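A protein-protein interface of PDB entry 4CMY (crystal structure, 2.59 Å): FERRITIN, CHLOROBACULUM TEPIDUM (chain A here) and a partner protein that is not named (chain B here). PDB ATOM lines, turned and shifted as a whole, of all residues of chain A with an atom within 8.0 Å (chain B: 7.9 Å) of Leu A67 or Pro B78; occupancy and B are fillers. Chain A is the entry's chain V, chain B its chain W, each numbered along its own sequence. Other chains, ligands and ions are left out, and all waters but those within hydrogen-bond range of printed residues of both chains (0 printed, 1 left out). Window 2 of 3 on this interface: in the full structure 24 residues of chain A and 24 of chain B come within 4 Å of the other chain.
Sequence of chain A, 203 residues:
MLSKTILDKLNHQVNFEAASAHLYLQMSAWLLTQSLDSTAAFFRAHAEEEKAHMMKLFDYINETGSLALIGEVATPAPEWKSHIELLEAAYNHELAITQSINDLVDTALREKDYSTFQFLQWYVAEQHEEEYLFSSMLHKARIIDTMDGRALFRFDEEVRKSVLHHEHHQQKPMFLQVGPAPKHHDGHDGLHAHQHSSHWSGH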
ATOM      1  N   LEU A   2     -17.440 -35.714  -5.362  1.00  0.00           N
ATOM      2  CA  LEU A   2     -16.212 -35.720  -6.199  1.00  0.00           C
ATOM      3  C   LEU A   2     -15.186 -34.722  -5.704  1.00  0.00           C
ATOM      4  O   LEU A   2     -15.520 -33.599  -5.417  1.00  0.00           O
ATOM      5  CB  LEU A   2     -16.531 -35.403  -7.663  1.00  0.00           C
ATOM      6  CG  LEU A   2     -17.159 -36.500  -8.522  1.00  0.00           C
ATOM      7  CD1 LEU A   2     -17.476 -35.921  -9.886  1.00  0.00           C
ATOM      8  CD2 LEU A   2     -16.246 -37.702  -8.677  1.00  0.00           C
ATOM      9  N   LEU A   7     -13.078 -33.903 -10.440  1.00  0.00           N
ATOM     10  CA  LEU A   7     -14.080 -33.086 -11.141  1.00  0.00           C
ATOM     11  C   LEU A   7     -13.490 -32.278 -12.292  1.00  0.00           C
ATOM     12  O   LEU A   7     -13.997 -32.331 -13.400  1.00  0.00           O
ATOM     13  CB  LEU A   7     -14.737 -32.092 -10.209  1.00  0.00           C
ATOM     14  CG  LEU A   7     -16.209 -31.711 -10.401  1.00  0.00           C
ATOM     15  CD1 LEU A   7     -16.438 -30.277  -9.942  1.00  0.00           C
ATOM     16  CD2 LEU A   7     -16.698 -31.900 -11.827  1.00  0.00           C
ATOM     17  N   ASP A   8     -12.375 -31.606 -12.058  1.00  0.00           N
ATOM     18  CA  ASP A   8     -11.779 -30.788 -13.112  1.00  0.00           C
ATOM     19  C   ASP A   8     -11.290 -31.622 -14.269  1.00  0.00           C
ATOM     20  O   ASP A   8     -11.449 -31.234 -15.437  1.00  0.00           O
ATOM     21  CB  ASP A   8     -10.645 -29.918 -12.591  1.00  0.00           C
ATOM     22  CG  ASP A   8     -11.151 -28.755 -11.704  1.00  0.00           C
ATOM     23  OD1 ASP A   8     -12.385 -28.495 -11.640  1.00  0.00           O
ATOM     24  OD2 ASP A   8     -10.287 -28.108 -11.052  1.00  0.00           O
ATOM     25  N   ASN A  11     -14.547 -32.977 -16.193  1.00  0.00           N
ATOM     26  CA  ASN A  11     -14.997 -31.881 -17.022  1.00  0.00           C
ATOM     27  C   ASN A  11     -14.044 -31.579 -18.175  1.00  0.00           C
ATOM     28  O   ASN A  11     -14.485 -31.218 -19.274  1.00  0.00           O
ATOM     29  CB  ASN A  11     -15.219 -30.633 -16.208  1.00  0.00           C
ATOM     30  CG  ASN A  11     -16.590 -30.595 -15.588  1.00  0.00           C
ATOM     31  OD1 ASN A  11     -17.524 -31.194 -16.088  1.00  0.00           O
ATOM     32  ND2 ASN A  11     -16.717 -29.903 -14.471  1.00  0.00           N
ATOM     33  N   VAL A  14     -15.077 -34.335 -20.618  1.00  0.00           N
ATOM     34  CA  VAL A  14     -16.298 -33.920 -21.278  1.00  0.00           C
ATOM     35  C   VAL A  14     -15.991 -33.004 -22.460  1.00  0.00           C
ATOM     36  O   VAL A  14     -16.445 -33.218 -23.570  1.00  0.00           O
ATOM     37  CB  VAL A  14     -17.232 -33.169 -20.347  1.00  0.00           C
ATOM     38  CG1 VAL A  14     -18.361 -32.535 -21.127  1.00  0.00           C
ATOM     39  CG2 VAL A  14     -17.827 -34.110 -19.321  1.00  0.00           C
ATOM     40  N   PHE A  58     -20.825 -36.628 -18.844  1.00  0.00           N
ATOM     41  CA  PHE A  58     -21.700 -35.525 -18.415  1.00  0.00           C
ATOM     42  C   PHE A  58     -22.727 -36.036 -17.413  1.00  0.00           C
ATOM     43  O   PHE A  58     -22.883 -35.465 -16.344  1.00  0.00           O
ATOM     44  CB  PHE A  58     -22.352 -34.972 -19.681  1.00  0.00           C
ATOM     45  CG  PHE A  58     -23.356 -33.885 -19.479  1.00  0.00           C
ATOM     46  CD1 PHE A  58     -24.717 -34.206 -19.306  1.00  0.00           C
ATOM     47  CD2 PHE A  58     -22.988 -32.561 -19.574  1.00  0.00           C
ATOM     48  CE1 PHE A  58     -25.666 -33.209 -19.176  1.00  0.00           C
ATOM     49  CE2 PHE A  58     -23.917 -31.558 -19.405  1.00  0.00           C
ATOM     50  CZ  PHE A  58     -25.259 -31.878 -19.208  1.00  0.00           C
ATOM     51  N   ILE A  61     -21.058 -37.155 -13.959  1.00  0.00           N
ATOM     52  CA  ILE A  61     -20.713 -36.007 -13.137  1.00  0.00           C
ATOM     53  C   ILE A  61     -21.952 -35.495 -12.454  1.00  0.00           C
ATOM     54  O   ILE A  61     -21.947 -35.299 -11.246  1.00  0.00           O
ATOM     55  CB  ILE A  61     -20.070 -34.888 -13.972  1.00  0.00           C
ATOM     56  CG1 ILE A  61     -18.697 -35.319 -14.490  1.00  0.00           C
ATOM     57  CG2 ILE A  61     -19.885 -33.642 -13.152  1.00  0.00           C
ATOM     58  CD1 ILE A  61     -18.266 -34.538 -15.721  1.00  0.00           C
ATOM     59  N   ASN A  62     -23.014 -35.262 -13.226  1.00  0.00           N
ATOM     60  CA  ASN A  62     -24.260 -34.719 -12.662  1.00  0.00           C
ATOM     61  C   ASN A  62     -24.906 -35.643 -11.638  1.00  0.00           C
ATOM     62  O   ASN A  62     -25.346 -35.184 -10.599  1.00  0.00           O
ATOM     63  CB  ASN A  62     -25.263 -34.370 -13.741  1.00  0.00           C
ATOM     64  CG  ASN A  62     -24.816 -33.206 -14.604  1.00  0.00           C
ATOM     65  OD1 ASN A  62     -24.058 -32.347 -14.166  1.00  0.00           O
ATOM     66  ND2 ASN A  62     -25.253 -33.199 -15.859  1.00  0.00           N
ATOM     67  N   GLU A  63     -24.858 -36.950 -11.874  1.00  0.00           N
ATOM     68  CA  GLU A  63     -25.373 -37.924 -10.909  1.00  0.00           C
ATOM     69  C   GLU A  63     -24.621 -37.880  -9.579  1.00  0.00           C
ATOM     70  O   GLU A  63     -25.231 -38.099  -8.537  1.00  0.00           O
ATOM     71  CB  GLU A  63     -25.325 -39.357 -11.470  1.00  0.00           C
ATOM     72  CG  GLU A  63     -26.355 -39.616 -12.546  1.00  0.00           C
ATOM     73  CD  GLU A  63     -26.136 -40.907 -13.339  1.00  0.00           C
ATOM     74  OE1 GLU A  63     -25.324 -41.768 -12.891  1.00  0.00           O
ATOM     75  OE2 GLU A  63     -26.840 -41.074 -14.383  1.00  0.00           O
ATOM     76  N   THR A  64     -23.312 -37.619  -9.590  1.00  0.00           N
ATOM     77  CA  THR A  64     -22.571 -37.520  -8.327  1.00  0.00           C
ATOM     78  C   THR A  64     -22.928 -36.285  -7.513  1.00  0.00           C
ATOM     79  O   THR A  64     -22.424 -36.102  -6.398  1.00  0.00           O
ATOM     80  CB  THR A  64     -21.029 -37.471  -8.520  1.00  0.00           C
ATOM     81  OG1 THR A  64     -20.637 -36.242  -9.154  1.00  0.00           O
ATOM     82  CG2 THR A  64     -20.531 -38.639  -9.318  1.00  0.00           C
ATOM     83  N   GLY A  65     -23.705 -35.370  -8.094  1.00  0.00           N
ATOM     84  CA  GLY A  65     -24.053 -34.116  -7.424  1.00  0.00           C
ATOM     85  C   GLY A  65     -23.199 -32.904  -7.777  1.00  0.00           C
ATOM     86  O   GLY A  65     -23.475 -31.821  -7.302  1.00  0.00           O
ATOM     87  N   SER A  66     -22.198 -33.051  -8.647  1.00  0.00           N
ATOM     88  CA  SER A  66     -21.466 -31.894  -9.170  1.00  0.00           C
ATOM     89  C   SER A  66     -22.087 -31.381 -10.450  1.00  0.00           C
ATOM     90  O   SER A  66     -22.978 -32.002 -11.025  1.00  0.00           O
ATOM     91  CB  SER A  66     -20.012 -32.260  -9.421  1.00  0.00           C
ATOM     92  OG  SER A  66     -19.394 -32.687  -8.227  1.00  0.00           O
ATOM     93  N   LEU A  67     -21.583 -30.250 -10.924  1.00  0.00           N
ATOM     94  CA  LEU A  67     -22.110 -29.620 -12.134  1.00  0.00           C
ATOM     95  C   LEU A  67     -21.172 -29.814 -13.307  1.00  0.00           C
ATOM     96  O   LEU A  67     -20.025 -29.368 -13.296  1.00  0.00           O
ATOM     97  CB  LEU A  67     -22.305 -28.145 -11.868  1.00  0.00           C
ATOM     98  CG  LEU A  67     -22.690 -27.251 -13.048  1.00  0.00           C
ATOM     99  CD1 LEU A  67     -24.117 -27.509 -13.501  1.00  0.00           C
ATOM    100  CD2 LEU A  67     -22.524 -25.806 -12.635  1.00  0.00           C
ATOM    101  N   ALA A  68     -21.641 -30.507 -14.320  1.00  0.00           N
ATOM    102  CA  ALA A  68     -20.806 -30.769 -15.488  1.00  0.00           C
ATOM    103  C   ALA A  68     -20.705 -29.477 -16.286  1.00  0.00           C
ATOM    104  O   ALA A  68     -21.652 -28.738 -16.376  1.00  0.00           O
ATOM    105  CB  ALA A  68     -21.396 -31.880 -16.335  1.00  0.00           C
ATOM    106  N   LEU A  69     -19.549 -29.273 -16.899  1.00  0.00           N
ATOM    107  CA  LEU A  69     -19.277 -28.073 -17.666  1.00  0.00           C
ATOM    108  C   LEU A  69     -18.786 -28.446 -19.039  1.00  0.00           C
ATOM    109  O   LEU A  69     -17.847 -29.248 -19.183  1.00  0.00           O
ATOM    110  CB  LEU A  69     -18.198 -27.243 -16.981  1.00  0.00           C
ATOM    111  CG  LEU A  69     -18.559 -26.695 -15.590  1.00  0.00           C
ATOM    112  CD1 LEU A  69     -17.346 -26.099 -14.900  1.00  0.00           C
ATOM    113  CD2 LEU A  69     -19.657 -25.675 -15.714  1.00  0.00           C
ATOM    114  N   ILE A  70     -19.398 -27.851 -20.056  1.00  0.00           N
ATOM    115  CA  ILE A  70     -19.007 -28.121 -21.425  1.00  0.00           C
ATOM    116  C   ILE A  70     -17.733 -27.381 -21.814  1.00  0.00           C
ATOM    117  O   ILE A  70     -16.879 -27.943 -22.522  1.00  0.00           O
ATOM    118  CB  ILE A  70     -20.107 -27.702 -22.404  1.00  0.00           C
ATOM    119  CG1 ILE A  70     -21.481 -28.247 -21.977  1.00  0.00           C
ATOM    120  CG2 ILE A  70     -19.785 -28.214 -23.817  1.00  0.00           C
ATOM    121  CD1 ILE A  70     -21.643 -29.754 -22.116  1.00  0.00           C
ATOM    122  N   LEU B  23     -25.519 -24.859 -25.106  1.00  0.00           N
ATOM    123  CA  LEU B  23     -26.176 -24.011 -24.154  1.00  0.00           C
ATOM    124  C   LEU B  23     -27.255 -24.773 -23.419  1.00  0.00           C
ATOM    125  O   LEU B  23     -27.333 -24.754 -22.197  1.00  0.00           O
ATOM    126  CB  LEU B  23     -26.775 -22.784 -24.833  1.00  0.00           C
ATOM    127  CG  LEU B  23     -27.535 -21.787 -23.914  1.00  0.00           C
ATOM    128  CD1 LEU B  23     -26.625 -21.206 -22.853  1.00  0.00           C
ATOM    129  CD2 LEU B  23     -28.171 -20.660 -24.709  1.00  0.00           C
ATOM    130  N   LEU B  25     -27.521 -28.060 -23.128  1.00  0.00           N
ATOM    131  CA  LEU B  25     -26.900 -29.074 -22.277  1.00  0.00           C
ATOM    132  C   LEU B  25     -26.497 -28.451 -20.942  1.00  0.00           C
ATOM    133  O   LEU B  25     -26.763 -29.005 -19.890  1.00  0.00           O
ATOM    134  CB  LEU B  25     -25.688 -29.664 -22.948  1.00  0.00           C
ATOM    135  CG  LEU B  25     -25.705 -31.089 -23.490  1.00  0.00           C
ATOM    136  CD1 LEU B  25     -27.074 -31.693 -23.655  1.00  0.00           C
ATOM    137  CD2 LEU B  25     -24.961 -31.134 -24.813  1.00  0.00           C
ATOM    138  N   GLN B  26     -25.878 -27.274 -21.011  1.00  0.00           N
ATOM    139  CA  GLN B  26     -25.398 -26.619 -19.811  1.00  0.00           C
ATOM    140  C   GLN B  26     -26.552 -26.219 -18.904  1.00  0.00           C
ATOM    141  O   GLN B  26     -26.452 -26.366 -17.683  1.00  0.00           O
ATOM    142  CB  GLN B  26     -24.542 -25.420 -20.164  1.00  0.00           C
ATOM    143  CG  GLN B  26     -23.769 -24.851 -19.023  1.00  0.00           C
ATOM    144  CD  GLN B  26     -22.799 -25.842 -18.431  1.00  0.00           C
ATOM    145  OE1 GLN B  26     -21.641 -25.939 -18.842  1.00  0.00           O
ATOM    146  NE2 GLN B  26     -23.244 -26.530 -17.385  1.00  0.00           N
ATOM    147  N   MET B  27     -27.647 -25.761 -19.501  1.00  0.00           N
ATOM    148  CA  MET B  27     -28.834 -25.429 -18.741  1.00  0.00           C
ATOM    149  C   MET B  27     -29.379 -26.670 -18.063  1.00  0.00           C
ATOM    150  O   MET B  27     -29.763 -26.636 -16.899  1.00  0.00           O
ATOM    151  CB  MET B  27     -29.908 -24.798 -19.633  1.00  0.00           C
ATOM    152  CG  MET B  27     -29.607 -23.374 -20.060  1.00  0.00           C
ATOM    153  SD  MET B  27     -30.880 -22.738 -21.185  1.00  0.00           S
ATOM    154  CE  MET B  27     -30.390 -21.033 -21.319  1.00  0.00           C
ATOM    155  N   SER B  28     -29.382 -27.776 -18.775  1.00  0.00           N
ATOM    156  CA  SER B  28     -29.849 -29.038 -18.215  1.00  0.00           C
ATOM    157  C   SER B  28     -29.083 -29.398 -16.978  1.00  0.00           C
ATOM    158  O   SER B  28     -29.664 -29.806 -15.961  1.00  0.00           O
ATOM    159  CB  SER B  28     -29.694 -30.175 -19.233  1.00  0.00           C
ATOM    160  OG  SER B  28     -30.257 -31.370 -18.744  1.00  0.00           O
ATOM    161  N   ALA B  29     -27.773 -29.259 -17.053  1.00  0.00           N
ATOM    162  CA  ALA B  29     -26.903 -29.600 -15.907  1.00  0.00           C
ATOM    163  C   ALA B  29     -27.206 -28.736 -14.676  1.00  0.00           C
ATOM    164  O   ALA B  29     -27.269 -29.240 -13.573  1.00  0.00           O
ATOM    165  CB  ALA B  29     -25.443 -29.477 -16.288  1.00  0.00           C
ATOM    166  N   TRP B  30     -27.386 -27.441 -14.889  1.00  0.00           N
ATOM    167  CA  TRP B  30     -27.700 -26.532 -13.816  1.00  0.00           C
ATOM    168  C   TRP B  30     -29.037 -26.916 -13.195  1.00  0.00           C
ATOM    169  O   TRP B  30     -29.183 -26.943 -11.975  1.00  0.00           O
ATOM    170  CB  TRP B  30     -27.742 -25.075 -14.331  1.00  0.00           C
ATOM    171  CG  TRP B  30     -28.027 -24.103 -13.259  1.00  0.00           C
ATOM    172  CD1 TRP B  30     -27.128 -23.591 -12.365  1.00  0.00           C
ATOM    173  CD2 TRP B  30     -29.298 -23.575 -12.897  1.00  0.00           C
ATOM    174  NE1 TRP B  30     -27.760 -22.786 -11.493  1.00  0.00           N
ATOM    175  CE2 TRP B  30     -29.099 -22.752 -11.784  1.00  0.00           C
ATOM    176  CE3 TRP B  30     -30.577 -23.729 -13.385  1.00  0.00           C
ATOM    177  CZ2 TRP B  30     -30.152 -22.057 -11.152  1.00  0.00           C
ATOM    178  CZ3 TRP B  30     -31.631 -23.032 -12.766  1.00  0.00           C
ATOM    179  CH2 TRP B  30     -31.410 -22.221 -11.660  1.00  0.00           C
ATOM    180  N   LEU B  31     -30.024 -27.169 -14.047  1.00  0.00           N
ATOM    181  CA  LEU B  31     -31.369 -27.497 -13.575  1.00  0.00           C
ATOM    182  C   LEU B  31     -31.359 -28.736 -12.681  1.00  0.00           C
ATOM    183  O   LEU B  31     -32.102 -28.789 -11.711  1.00  0.00           O
ATOM    184  CB  LEU B  31     -32.334 -27.700 -14.751  1.00  0.00           C
ATOM    185  CG  LEU B  31     -32.677 -26.406 -15.474  1.00  0.00           C
ATOM    186  CD1 LEU B  31     -33.205 -26.682 -16.871  1.00  0.00           C
ATOM    187  CD2 LEU B  31     -33.695 -25.624 -14.665  1.00  0.00           C
ATOM    188  N   LEU B  32     -30.513 -29.704 -12.999  1.00  0.00           N
ATOM    189  CA  LEU B  32     -30.384 -30.856 -12.130  1.00  0.00           C
ATOM    190  C   LEU B  32     -29.906 -30.451 -10.717  1.00  0.00           C
ATOM    191  O   LEU B  32     -30.372 -31.033  -9.742  1.00  0.00           O
ATOM    192  CB  LEU B  32     -29.469 -31.927 -12.707  1.00  0.00           C
ATOM    193  CG  LEU B  32     -30.065 -32.678 -13.894  1.00  0.00           C
ATOM    194  CD1 LEU B  32     -29.013 -33.503 -14.616  1.00  0.00           C
ATOM    195  CD2 LEU B  32     -31.220 -33.553 -13.507  1.00  0.00           C
ATOM    196  N   THR B  33     -29.029 -29.451 -10.591  1.00  0.00           N
ATOM    197  CA  THR B  33     -28.585 -29.002  -9.244  1.00  0.00           C
ATOM    198  C   THR B  33     -29.694 -28.361  -8.453  1.00  0.00           C
ATOM    199  O   THR B  33     -29.596 -28.289  -7.256  1.00  0.00           O
ATOM    200  CB  THR B  33     -27.386 -28.032  -9.266  1.00  0.00           C
ATOM    201  OG1 THR B  33     -27.797 -26.756  -9.752  1.00  0.00           O
ATOM    202  CG2 THR B  33     -26.248 -28.569 -10.141  1.00  0.00           C
ATOM    203  N   THR B  75     -19.287 -21.937 -24.335  1.00  0.00           N
ATOM    204  CA  THR B  75     -20.458 -21.963 -23.485  1.00  0.00           C
ATOM    205  C   THR B  75     -20.065 -21.436 -22.136  1.00  0.00           C
ATOM    206  O   THR B  75     -19.267 -22.068 -21.429  1.00  0.00           O
ATOM    207  CB  THR B  75     -21.024 -23.384 -23.335  1.00  0.00           C
ATOM    208  OG1 THR B  75     -21.199 -23.948 -24.639  1.00  0.00           O
ATOM    209  CG2 THR B  75     -22.348 -23.362 -22.594  1.00  0.00           C
ATOM    210  N   PRO B  76     -20.615 -20.271 -21.766  1.00  0.00           N
ATOM    211  CA  PRO B  76     -20.322 -19.759 -20.429  1.00  0.00           C
ATOM    212  C   PRO B  76     -20.859 -20.691 -19.334  1.00  0.00           C
ATOM    213  O   PRO B  76     -21.891 -21.372 -19.523  1.00  0.00           O
ATOM    214  CB  PRO B  76     -21.036 -18.402 -20.402  1.00  0.00           C
ATOM    215  CG  PRO B  76     -22.177 -18.560 -21.361  1.00  0.00           C
ATOM    216  CD  PRO B  76     -21.708 -19.528 -22.424  1.00  0.00           C
ATOM    217  N   ALA B  77     -20.150 -20.713 -18.207  1.00  0.00           N
ATOM    218  CA  ALA B  77     -20.613 -21.427 -17.004  1.00  0.00           C
ATOM    219  C   ALA B  77     -21.990 -20.886 -16.583  1.00  0.00           C
ATOM    220  O   ALA B  77     -22.370 -19.806 -16.984  1.00  0.00           O
ATOM    221  CB  ALA B  77     -19.593 -21.305 -15.864  1.00  0.00           C
ATOM    222  N   PRO B  78     -22.755 -21.668 -15.828  1.00  0.00           N
ATOM    223  CA  PRO B  78     -24.093 -21.258 -15.446  1.00  0.00           C
ATOM    224  C   PRO B  78     -24.176 -20.092 -14.483  1.00  0.00           C
ATOM    225  O   PRO B  78     -23.812 -20.215 -13.324  1.00  0.00           O
ATOM    226  CB  PRO B  78     -24.635 -22.480 -14.760  1.00  0.00           C
ATOM    227  CG  PRO B  78     -23.924 -23.589 -15.417  1.00  0.00           C
ATOM    228  CD  PRO B  78     -22.527 -23.089 -15.556  1.00  0.00           C
ATOM    229  N   GLU B  79     -24.600 -18.938 -14.974  1.00  0.00           N
ATOM    230  CA  GLU B  79     -24.751 -17.763 -14.109  1.00  0.00           C
ATOM    231  C   GLU B  79     -26.087 -17.823 -13.329  1.00  0.00           C
ATOM    232  O   GLU B  79     -26.203 -17.200 -12.290  1.00  0.00           O
ATOM    233  CB  GLU B  79     -24.645 -16.472 -14.949  1.00  0.00           C
ATOM    234  N   TRP B  80     -27.067 -18.595 -13.814  1.00  0.00           N
ATOM    235  CA  TRP B  80     -28.483 -18.318 -13.525  1.00  0.00           C
ATOM    236  C   TRP B  80     -28.817 -18.345 -12.042  1.00  0.00           C
ATOM    237  O   TRP B  80     -28.417 -19.253 -11.340  1.00  0.00           O
ATOM    238  CB  TRP B  80     -29.410 -19.265 -14.328  1.00  0.00           C
ATOM    239  CG  TRP B  80     -29.057 -19.241 -15.777  1.00  0.00           C
ATOM    240  CD1 TRP B  80     -29.279 -18.220 -16.678  1.00  0.00           C
ATOM    241  CD2 TRP B  80     -28.357 -20.252 -16.483  1.00  0.00           C
ATOM    242  NE1 TRP B  80     -28.761 -18.562 -17.908  1.00  0.00           N
ATOM    243  CE2 TRP B  80     -28.199 -19.803 -17.812  1.00  0.00           C
ATOM    244  CE3 TRP B  80     -27.867 -21.495 -16.125  1.00  0.00           C
ATOM    245  CZ2 TRP B  80     -27.555 -20.559 -18.777  1.00  0.00           C
ATOM    246  CZ3 TRP B  80     -27.186 -22.261 -17.091  1.00  0.00           C
ATOM    247  CH2 TRP B  80     -27.024 -21.793 -18.389  1.00  0.00           C
ATOM    248  N   LYS B  81     -29.567 -17.336 -11.597  1.00  0.00           N
ATOM    249  CA  LYS B  81     -29.954 -17.191 -10.197  1.00  0.00           C
ATOM    250  C   LYS B  81     -31.291 -17.879  -9.924  1.00  0.00           C
ATOM    251  O   LYS B  81     -31.554 -18.294  -8.806  1.00  0.00           O
ATOM    252  CB  LYS B  81     -30.017 -15.704  -9.809  1.00  0.00           C
ATOM    253  N   GLU B  85     -34.920 -16.913 -14.662  1.00  0.00           N
ATOM    254  CA  GLU B  85     -33.855 -16.207 -15.350  1.00  0.00           C
ATOM    255  C   GLU B  85     -33.348 -17.098 -16.513  1.00  0.00           C
ATOM    256  O   GLU B  85     -33.046 -16.616 -17.617  1.00  0.00           O
ATOM    257  CB  GLU B  85     -32.768 -15.805 -14.345  1.00  0.00           C
ATOM    258  CG  GLU B  85     -31.761 -14.756 -14.834  1.00  0.00           C
ATOM    259  CD  GLU B  85     -30.497 -14.656 -13.954  1.00  0.00           C
ATOM    260  OE1 GLU B  85     -30.641 -14.737 -12.706  1.00  0.00           O
ATOM    261  OE2 GLU B  85     -29.364 -14.500 -14.519  1.00  0.00           O
ATOM    262  N   LEU B  86     -33.274 -18.399 -16.273  1.00  0.00           N
ATOM    263  CA  LEU B  86     -32.787 -19.345 -17.295  1.00  0.00           C
ATOM    264  C   LEU B  86     -33.761 -19.444 -18.453  1.00  0.00           C
ATOM    265  O   LEU B  86     -33.352 -19.408 -19.607  1.00  0.00           O
ATOM    266  CB  LEU B  86     -32.449 -20.695 -16.653  1.00  0.00           C
ATOM    267  CG  LEU B  86     -32.646 -22.117 -17.154  1.00  0.00           C
ATOM    268  CD1 LEU B  86     -33.045 -22.320 -18.590  1.00  0.00           C
ATOM    269  CD2 LEU B  86     -31.387 -22.921 -16.839  1.00  0.00           C
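Leu A67 touches just these residues of chain B: Ala B29 (3.5 Å), Trp B30 (3.6 Å) and Pro B78 (3.8 Å).
Printed residues of chain B within 4 Å of Ala A68: Gln B26 and Ala B29.
Of the printed residues of chain B, Ile A70 touches Gln B26.
Printed residues of chain A within 4 Å of Leu B32: Asn A62 (3.9 Å).
Pro B78 touches just these residues of chain A: Leu A67 and Leu A69.
The nearest residue of chain A that does not touch Pro B78 is Ala A68 (5.7 Å).
The nearest printed residue of chain A that does not touch Trp B30 is Asn A62 (6.0 Å).
The side-chain amide nitrogen of Gln B26 sits at hydrogen-bond distance from the backbone carbonyl oxygen of Ala A68, at 2.9 Å.
The side-chain amide oxygen of Gln B26 is in hydrogen-bond range of the backbone NH of Ile A70 (3.2 Å).
The backbone carbonyl oxygen (O) of Trp B30 sits at hydrogen-bond distance from the side-chain hydroxyl (OG1) of Thr B33 (2.6 Å).
N of Leu A69 is in hydrogen-bond range of OD1 of Asn A11 (2.9 Å).
ND2 of Asn A62 lies within hydrogen-bond range of O of Phe A58, 3.3 Å away.
The side-chain amide oxygen of Asn A62 sits close to the backbone carbonyl oxygen of Ser A66, at 3.3 Å.
The backbone NH (N) of Ala A68 is in hydrogen-bond range of the side-chain amide oxygen (OD1) of Asn A62.
Phe A58 touches Leu B25.
Phe A58 touches Ala B29 (CZ to CB, 3.8 Å).
Ala B29 touches Asn A62 (CB to ND2, 3.8 Å).
CB of Asn A62 touches CD1 of Leu B32 (3.9 Å).
CD1 of Leu A67 touches C of Ala B29 (3.5 Å).
CD1 of Leu A67 touches N of Trp B30, at 3.6 Å.
CD2 of Leu A67 touches CG of Pro B78, 3.8 Å away.
CB of Ala B29 touches O of Ala A68 (3.9 Å).
CA of Leu A69 touches OE1 of Gln B26 (3.4 Å).
CD of Pro B78 touches CD2 of Leu A69, at 3.9 Å.
Of the 16 printed residues of chain A, 6 touch a printed residue of chain B.
Of the 19 printed residues of chain B, 6 touch a printed residue of chain A.
Hydrophobic or aromatic side chains of chain B that line the printed part of chain A: Ala B29, Leu B32 and Pro B78.
Among the printed residues, no Asp or Glu carboxylate lies within 4 Å of a Lys or Arg side-chain nitrogen of the other chain.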
